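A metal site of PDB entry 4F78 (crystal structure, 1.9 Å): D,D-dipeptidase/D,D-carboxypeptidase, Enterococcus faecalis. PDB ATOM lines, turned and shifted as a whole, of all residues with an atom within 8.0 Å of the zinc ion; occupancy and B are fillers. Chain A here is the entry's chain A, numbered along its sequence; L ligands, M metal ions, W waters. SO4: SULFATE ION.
The zinc ion is bound by OD1 of Asp 115 (2.2 Å), ND1 of His 168 (2.2 Å), water W1 (2.2 Å), NE2 of His 108 (2.2 Å) and OD2 of Asp 115 (2.6 Å).
Slightly farther from the zinc ion lies an oxygen (O2) of the ligand (2.7 Å).
Within 4 Å of the zinc ion: His 108, Asp 115 and His 168.
The nearest printed residue that does not touch the zinc ion is Glu 165 (4.2 Å).
Water W1 lies within hydrogen-bond range of the side-chain carboxylate of Glu 165 (2.5 Å) and the indole nitrogen of Trp 167 (3.0 Å).
The backbone carbonyl oxygen of His 108 sits at hydrogen-bond distance from the backbone NH of Arg 75 (3.1 Å).
N of Asp 115 lies within hydrogen-bond range of O of Ser 72 (2.8 Å).
The backbone NH of His 108 sits close to the side-chain hydroxyl of Ser 106, at 3.2 Å.
The backbone carbonyl oxygen (O) of His 168 sits at hydrogen-bond distance from the backbone NH (N) of Arg 151.
OD2 of Asp 115 sits close to NH2 of Arg 75 (3.3 Å).
The backbone carbonyl oxygen of Gly 73 lies within hydrogen-bond range of a ring nitrogen (ND1) of His 108 (2.6 Å).
A ring nitrogen (NE2) of His 168 lies within hydrogen-bond range of the side-chain carboxylate (OE1) of Glu 107, 2.8 Å away.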
ATOM      1  N   SER A  72      19.143 -13.136  25.557  1.00  0.00           N
ATOM      2  CA  SER A  72      18.881 -14.581  25.599  1.00  0.00           C
ATOM      3  C   SER A  72      19.696 -15.244  24.519  1.00  0.00           C
ATOM      4  O   SER A  72      19.799 -14.736  23.399  1.00  0.00           O
ATOM      5  CB  SER A  72      17.408 -14.904  25.331  1.00  0.00           C
ATOM      6  OG  SER A  72      17.121 -16.227  25.759  1.00  0.00           O
ATOM      7  N   GLY A  73      20.271 -16.394  24.834  1.00  0.00           N
ATOM      8  CA  GLY A  73      21.028 -17.123  23.814  1.00  0.00           C
ATOM      9  C   GLY A  73      20.439 -18.542  23.755  1.00  0.00           C
ATOM     10  O   GLY A  73      19.259 -18.702  23.415  1.00  0.00           O
ATOM     11  N   ARG A  75      18.534 -21.699  24.876  1.00  0.00           N
ATOM     12  CA  ARG A  75      17.499 -22.067  25.868  1.00  0.00           C
ATOM     13  C   ARG A  75      17.275 -23.563  25.768  1.00  0.00           C
ATOM     14  O   ARG A  75      17.191 -24.110  24.666  1.00  0.00           O
ATOM     15  CB  ARG A  75      16.186 -21.388  25.506  1.00  0.00           C
ATOM     16  CG  ARG A  75      16.156 -19.877  25.803  1.00  0.00           C
ATOM     17  CD  ARG A  75      14.841 -19.340  25.234  1.00  0.00           C
ATOM     18  NE  ARG A  75      14.856 -17.883  25.208  1.00  0.00           N
ATOM     19  CZ  ARG A  75      14.025 -17.155  24.495  1.00  0.00           C
ATOM     20  NH1 ARG A  75      13.077 -17.756  23.767  1.00  0.00           N
ATOM     21  NH2 ARG A  75      14.095 -15.835  24.551  1.00  0.00           N
ATOM     22  N   GLN A  80      12.317 -22.887  27.362  1.00  0.00           N
ATOM     23  CA  GLN A  80      11.410 -22.397  26.312  1.00  0.00           C
ATOM     24  C   GLN A  80       9.928 -22.661  26.715  1.00  0.00           C
ATOM     25  O   GLN A  80       9.044 -21.830  26.458  1.00  0.00           O
ATOM     26  CB  GLN A  80      11.775 -23.021  24.954  1.00  0.00           C
ATOM     27  CG  GLN A  80      10.974 -22.496  23.780  1.00  0.00           C
ATOM     28  CD  GLN A  80      11.367 -21.028  23.462  1.00  0.00           C
ATOM     29  OE1 GLN A  80      12.453 -20.546  23.821  1.00  0.00           O
ATOM     30  NE2 GLN A  80      10.505 -20.334  22.748  1.00  0.00           N
ATOM     31  N   TYR A  99       4.984 -14.066  19.032  1.00  0.00           N
ATOM     32  CA  TYR A  99       6.297 -13.616  19.494  1.00  0.00           C
ATOM     33  C   TYR A  99       7.119 -14.673  20.218  1.00  0.00           C
ATOM     34  O   TYR A  99       8.290 -14.427  20.503  1.00  0.00           O
ATOM     35  CB  TYR A  99       6.192 -12.390  20.416  1.00  0.00           C
ATOM     36  CG  TYR A  99       5.832 -11.135  19.657  1.00  0.00           C
ATOM     37  CD1 TYR A  99       6.818 -10.384  19.011  1.00  0.00           C
ATOM     38  CD2 TYR A  99       4.522 -10.705  19.545  1.00  0.00           C
ATOM     39  CE1 TYR A  99       6.495  -9.243  18.284  1.00  0.00           C
ATOM     40  CE2 TYR A  99       4.200  -9.531  18.791  1.00  0.00           C
ATOM     41  CZ  TYR A  99       5.193  -8.828  18.187  1.00  0.00           C
ATOM     42  OH  TYR A  99       4.894  -7.683  17.439  1.00  0.00           O
ATOM     43  N   VAL A 100       6.507 -15.788  20.601  1.00  0.00           N
ATOM     44  CA  VAL A 100       7.293 -16.782  21.327  1.00  0.00           C
ATOM     45  C   VAL A 100       7.208 -18.080  20.560  1.00  0.00           C
ATOM     46  O   VAL A 100       6.100 -18.633  20.329  1.00  0.00           O
ATOM     47  CB  VAL A 100       6.833 -16.962  22.779  1.00  0.00           C
ATOM     48  CG1 VAL A 100       7.719 -18.005  23.501  1.00  0.00           C
ATOM     49  CG2 VAL A 100       6.890 -15.617  23.562  1.00  0.00           C
ATOM     50  N   ALA A 101       8.352 -18.592  20.111  1.00  0.00           N
ATOM     51  CA  ALA A 101       8.303 -19.858  19.368  1.00  0.00           C
ATOM     52  C   ALA A 101       7.771 -21.028  20.248  1.00  0.00           C
ATOM     53  O   ALA A 101       8.073 -21.065  21.438  1.00  0.00           O
ATOM     54  CB  ALA A 101       9.690 -20.174  18.857  1.00  0.00           C
ATOM     55  N   SER A 106      11.838 -23.514  18.543  1.00  0.00           N
ATOM     56  CA  SER A 106      12.598 -22.301  18.797  1.00  0.00           C
ATOM     57  C   SER A 106      14.048 -22.431  18.373  1.00  0.00           C
ATOM     58  O   SER A 106      14.762 -23.381  18.828  1.00  0.00           O
ATOM     59  CB  SER A 106      12.627 -22.044  20.307  1.00  0.00           C
ATOM     60  OG  SER A 106      13.359 -20.834  20.556  1.00  0.00           O
ATOM     61  N   GLU A 107      14.525 -21.489  17.552  1.00  0.00           N
ATOM     62  CA  GLU A 107      15.946 -21.467  17.167  1.00  0.00           C
ATOM     63  C   GLU A 107      16.839 -21.299  18.378  1.00  0.00           C
ATOM     64  O   GLU A 107      18.038 -21.657  18.331  1.00  0.00           O
ATOM     65  CB  GLU A 107      16.264 -20.237  16.284  1.00  0.00           C
ATOM     66  CG  GLU A 107      15.547 -20.141  15.035  1.00  0.00           C
ATOM     67  CD  GLU A 107      16.209 -19.122  14.102  1.00  0.00           C
ATOM     68  OE1 GLU A 107      16.512 -17.988  14.591  1.00  0.00           O
ATOM     69  OE2 GLU A 107      16.416 -19.463  12.898  1.00  0.00           O
ATOM     70  N   HIS A 108      16.326 -20.720  19.469  1.00  0.00           N
ATOM     71  CA  HIS A 108      17.155 -20.620  20.679  1.00  0.00           C
ATOM     72  C   HIS A 108      17.605 -21.963  21.188  1.00  0.00           C
ATOM     73  O   HIS A 108      18.671 -22.105  21.856  1.00  0.00           O
ATOM     74  CB  HIS A 108      16.397 -19.865  21.796  1.00  0.00           C
ATOM     75  CG  HIS A 108      16.365 -18.394  21.559  1.00  0.00           C
ATOM     76  ND1 HIS A 108      17.401 -17.563  21.944  1.00  0.00           N
ATOM     77  CD2 HIS A 108      15.459 -17.606  20.934  1.00  0.00           C
ATOM     78  CE1 HIS A 108      17.133 -16.322  21.562  1.00  0.00           C
ATOM     79  NE2 HIS A 108      15.960 -16.332  20.964  1.00  0.00           N
ATOM     80  N   ALA A 113      21.065 -18.903  17.944  1.00  0.00           N
ATOM     81  CA  ALA A 113      20.248 -17.692  17.918  1.00  0.00           C
ATOM     82  C   ALA A 113      20.490 -16.858  19.161  1.00  0.00           C
ATOM     83  O   ALA A 113      20.733 -17.411  20.240  1.00  0.00           O
ATOM     84  CB  ALA A 113      18.753 -18.036  17.852  1.00  0.00           C
ATOM     85  N   ILE A 114      20.412 -15.534  19.024  1.00  0.00           N
ATOM     86  CA  ILE A 114      20.684 -14.621  20.129  1.00  0.00           C
ATOM     87  C   ILE A 114      19.711 -13.463  20.074  1.00  0.00           C
ATOM     88  O   ILE A 114      19.396 -12.962  18.980  1.00  0.00           O
ATOM     89  CB  ILE A 114      22.178 -14.138  20.136  1.00  0.00           C
ATOM     90  CG1 ILE A 114      22.443 -13.240  21.375  1.00  0.00           C
ATOM     91  CG2 ILE A 114      22.494 -13.285  18.903  1.00  0.00           C
ATOM     92  CD1 ILE A 114      23.071 -13.932  22.476  1.00  0.00           C
ATOM     93  N   ASP A 115      19.187 -13.071  21.239  1.00  0.00           N
ATOM     94  CA  ASP A 115      18.363 -11.862  21.380  1.00  0.00           C
ATOM     95  C   ASP A 115      19.247 -10.759  21.945  1.00  0.00           C
ATOM     96  O   ASP A 115      19.878 -10.957  22.995  1.00  0.00           O
ATOM     97  CB  ASP A 115      17.198 -12.128  22.353  1.00  0.00           C
ATOM     98  CG  ASP A 115      16.104 -12.987  21.703  1.00  0.00           C
ATOM     99  OD1 ASP A 115      16.151 -13.105  20.436  1.00  0.00           O
ATOM    100  OD2 ASP A 115      15.269 -13.572  22.426  1.00  0.00           O
ATOM    101  N   LEU A 116      19.349  -9.610  21.254  1.00  0.00           N
ATOM    102  CA  LEU A 116      20.256  -8.524  21.714  1.00  0.00           C
ATOM    103  C   LEU A 116      19.448  -7.301  22.119  1.00  0.00           C
ATOM    104  O   LEU A 116      18.343  -7.080  21.584  1.00  0.00           O
ATOM    105  CB  LEU A 116      21.222  -8.111  20.595  1.00  0.00           C
ATOM    106  CG  LEU A 116      22.111  -9.296  20.136  1.00  0.00           C
ATOM    107  CD1 LEU A 116      22.860  -8.911  18.839  1.00  0.00           C
ATOM    108  CD2 LEU A 116      23.121  -9.618  21.248  1.00  0.00           C
ATOM    109  N   PHE A 125      12.607  -8.781  28.645  1.00  0.00           N
ATOM    110  CA  PHE A 125      13.127 -10.055  28.181  1.00  0.00           C
ATOM    111  C   PHE A 125      12.492 -10.478  26.846  1.00  0.00           C
ATOM    112  O   PHE A 125      13.179 -10.905  25.903  1.00  0.00           O
ATOM    113  CB  PHE A 125      12.865 -11.100  29.265  1.00  0.00           C
ATOM    114  CG  PHE A 125      13.313 -12.475  28.887  1.00  0.00           C
ATOM    115  CD1 PHE A 125      14.648 -12.872  29.113  1.00  0.00           C
ATOM    116  CD2 PHE A 125      12.408 -13.385  28.325  1.00  0.00           C
ATOM    117  CE1 PHE A 125      15.084 -14.163  28.763  1.00  0.00           C
ATOM    118  CE2 PHE A 125      12.826 -14.654  27.979  1.00  0.00           C
ATOM    119  CZ  PHE A 125      14.177 -15.054  28.193  1.00  0.00           C
ATOM    120  N   ILE A 126      11.175 -10.375  26.746  1.00  0.00           N
ATOM    121  CA  ILE A 126      10.498 -10.874  25.530  1.00  0.00           C
ATOM    122  C   ILE A 126      10.687  -9.903  24.347  1.00  0.00           C
ATOM    123  O   ILE A 126      10.877 -10.343  23.199  1.00  0.00           O
ATOM    124  CB  ILE A 126       8.994 -11.141  25.816  1.00  0.00           C
ATOM    125  CG1 ILE A 126       8.830 -12.434  26.618  1.00  0.00           C
ATOM    126  CG2 ILE A 126       8.197 -11.255  24.532  1.00  0.00           C
ATOM    127  CD1 ILE A 126       7.435 -13.016  26.587  1.00  0.00           C
ATOM    128  N   PRO A 128      13.332  -7.050  23.832  1.00  0.00           N
ATOM    129  CA  PRO A 128      14.392  -6.077  24.191  1.00  0.00           C
ATOM    130  C   PRO A 128      14.492  -4.957  23.137  1.00  0.00           C
ATOM    131  O   PRO A 128      14.084  -5.153  21.969  1.00  0.00           O
ATOM    132  CB  PRO A 128      15.671  -6.940  24.242  1.00  0.00           C
ATOM    133  CG  PRO A 128      15.349  -8.177  23.421  1.00  0.00           C
ATOM    134  CD  PRO A 128      13.855  -8.386  23.459  1.00  0.00           C
ATOM    135  N   ARG A 151      16.485 -12.499  11.888  1.00  0.00           N
ATOM    136  CA  ARG A 151      15.698 -13.663  11.513  1.00  0.00           C
ATOM    137  C   ARG A 151      14.267 -13.368  11.058  1.00  0.00           C
ATOM    138  O   ARG A 151      13.755 -13.994  10.076  1.00  0.00           O
ATOM    139  CB  ARG A 151      15.678 -14.619  12.704  1.00  0.00           C
ATOM    140  CG  ARG A 151      14.969 -15.920  12.407  1.00  0.00           C
ATOM    141  CD  ARG A 151      15.664 -16.689  11.293  1.00  0.00           C
ATOM    142  NE  ARG A 151      15.019 -18.002  11.125  1.00  0.00           N
ATOM    143  CZ  ARG A 151      13.930 -18.220  10.387  1.00  0.00           C
ATOM    144  NH1 ARG A 151      13.397 -17.213   9.682  1.00  0.00           N
ATOM    145  NH2 ARG A 151      13.430 -19.464  10.263  1.00  0.00           N
ATOM    146  N   TYR A 152      13.642 -12.409  11.726  1.00  0.00           N
ATOM    147  CA  TYR A 152      12.202 -12.183  11.576  1.00  0.00           C
ATOM    148  C   TYR A 152      11.921 -10.768  11.145  1.00  0.00           C
ATOM    149  O   TYR A 152      11.788  -9.859  11.995  1.00  0.00           O
ATOM    150  CB  TYR A 152      11.485 -12.443  12.917  1.00  0.00           C
ATOM    151  CG  TYR A 152      11.686 -13.864  13.429  1.00  0.00           C
ATOM    152  CD1 TYR A 152      11.292 -14.982  12.683  1.00  0.00           C
ATOM    153  CD2 TYR A 152      12.281 -14.095  14.684  1.00  0.00           C
ATOM    154  CE1 TYR A 152      11.500 -16.299  13.159  1.00  0.00           C
ATOM    155  CE2 TYR A 152      12.494 -15.399  15.163  1.00  0.00           C
ATOM    156  CZ  TYR A 152      12.082 -16.486  14.418  1.00  0.00           C
ATOM    157  OH  TYR A 152      12.301 -17.746  14.928  1.00  0.00           O
ATOM    158  N   ILE A 162       6.235 -15.677  12.461  1.00  0.00           N
ATOM    159  CA  ILE A 162       6.574 -14.982  13.687  1.00  0.00           C
ATOM    160  C   ILE A 162       6.559 -13.485  13.345  1.00  0.00           C
ATOM    161  O   ILE A 162       7.057 -13.072  12.248  1.00  0.00           O
ATOM    162  CB  ILE A 162       7.985 -15.432  14.157  1.00  0.00           C
ATOM    163  CG1 ILE A 162       7.984 -16.910  14.612  1.00  0.00           C
ATOM    164  CG2 ILE A 162       8.558 -14.521  15.266  1.00  0.00           C
ATOM    165  CD1 ILE A 162       7.222 -17.210  15.883  1.00  0.00           C
ATOM    166  N   GLU A 165      10.711  -8.982  14.606  1.00  0.00           N
ATOM    167  CA  GLU A 165      11.550  -8.793  15.824  1.00  0.00           C
ATOM    168  C   GLU A 165      12.879  -8.117  15.490  1.00  0.00           C
ATOM    169  O   GLU A 165      13.810  -8.742  14.948  1.00  0.00           O
ATOM    170  CB  GLU A 165      11.774 -10.151  16.560  1.00  0.00           C
ATOM    171  CG  GLU A 165      10.452 -10.866  16.932  1.00  0.00           C
ATOM    172  CD  GLU A 165      10.630 -12.195  17.666  1.00  0.00           C
ATOM    173  OE1 GLU A 165      11.787 -12.694  17.793  1.00  0.00           O
ATOM    174  OE2 GLU A 165       9.602 -12.734  18.174  1.00  0.00           O
ATOM    175  N   TRP A 167      15.213  -7.636  17.348  1.00  0.00           N
ATOM    176  CA  TRP A 167      16.323  -7.930  18.260  1.00  0.00           C
ATOM    177  C   TRP A 167      16.902  -9.342  18.131  1.00  0.00           C
ATOM    178  O   TRP A 167      17.899  -9.670  18.770  1.00  0.00           O
ATOM    179  CB  TRP A 167      15.817  -7.743  19.701  1.00  0.00           C
ATOM    180  CG  TRP A 167      14.612  -8.669  19.948  1.00  0.00           C
ATOM    181  CD1 TRP A 167      14.647 -10.040  20.194  1.00  0.00           C
ATOM    182  CD2 TRP A 167      13.214  -8.316  19.873  1.00  0.00           C
ATOM    183  NE1 TRP A 167      13.361 -10.529  20.307  1.00  0.00           N
ATOM    184  CE2 TRP A 167      12.461  -9.494  20.110  1.00  0.00           C
ATOM    185  CE3 TRP A 167      12.524  -7.114  19.627  1.00  0.00           C
ATOM    186  CZ2 TRP A 167      11.055  -9.502  20.128  1.00  0.00           C
ATOM    187  CZ3 TRP A 167      11.118  -7.123  19.645  1.00  0.00           C
ATOM    188  CH2 TRP A 167      10.409  -8.315  19.894  1.00  0.00           C
ATOM    189  N   HIS A 168      16.280 -10.176  17.297  1.00  0.00           N
ATOM    190  CA  HIS A 168      16.598 -11.602  17.206  1.00  0.00           C
ATOM    191  C   HIS A 168      17.435 -11.909  15.985  1.00  0.00           C
ATOM    192  O   HIS A 168      16.996 -11.724  14.841  1.00  0.00           O
ATOM    193  CB  HIS A 168      15.298 -12.438  17.222  1.00  0.00           C
ATOM    194  CG  HIS A 168      15.500 -13.929  17.090  1.00  0.00           C
ATOM    195  ND1 HIS A 168      15.027 -14.802  18.039  1.00  0.00           N
ATOM    196  CD2 HIS A 168      16.032 -14.680  16.110  1.00  0.00           C
ATOM    197  CE1 HIS A 168      15.302 -16.044  17.675  1.00  0.00           C
ATOM    198  NE2 HIS A 168      15.915 -15.998  16.495  1.00  0.00           N
ATOM    199  N   PHE A 169      18.662 -12.394  16.225  1.00  0.00           N
ATOM    200  CA  PHE A 169      19.628 -12.686  15.164  1.00  0.00           C
ATOM    201  C   PHE A 169      20.002 -14.162  15.131  1.00  0.00           C
ATOM    202  O   PHE A 169      20.106 -14.836  16.169  1.00  0.00           O
ATOM    203  CB  PHE A 169      20.882 -11.844  15.344  1.00  0.00           C
ATOM    204  CG  PHE A 169      20.641 -10.431  14.988  1.00  0.00           C
ATOM    205  CD1 PHE A 169      20.087  -9.560  15.920  1.00  0.00           C
ATOM    206  CD2 PHE A 169      20.887  -9.987  13.702  1.00  0.00           C
ATOM    207  CE1 PHE A 169      19.803  -8.220  15.576  1.00  0.00           C
ATOM    208  CE2 PHE A 169      20.619  -8.651  13.346  1.00  0.00           C
ATOM    209  CZ  PHE A 169      20.068  -7.772  14.299  1.00  0.00           C
HETATM  210  S   SO4 L   1      11.966 -17.272  20.365  1.00  0.00           S
HETATM  211  O1  SO4 L   1      10.619 -17.381  20.931  1.00  0.00           O
HETATM  212  O2  SO4 L   1      12.765 -16.334  21.189  1.00  0.00           O
HETATM  213  O3  SO4 L   1      12.492 -18.638  20.339  1.00  0.00           O
HETATM  214  O4  SO4 L   1      12.081 -16.789  19.005  1.00  0.00           O
HETATM  215 ZN    ZN M   1      14.661 -14.678  20.203  1.00  0.00          ZN
HETATM  216  O   HOH W   1      12.861 -13.435  19.974  1.00  0.00           O
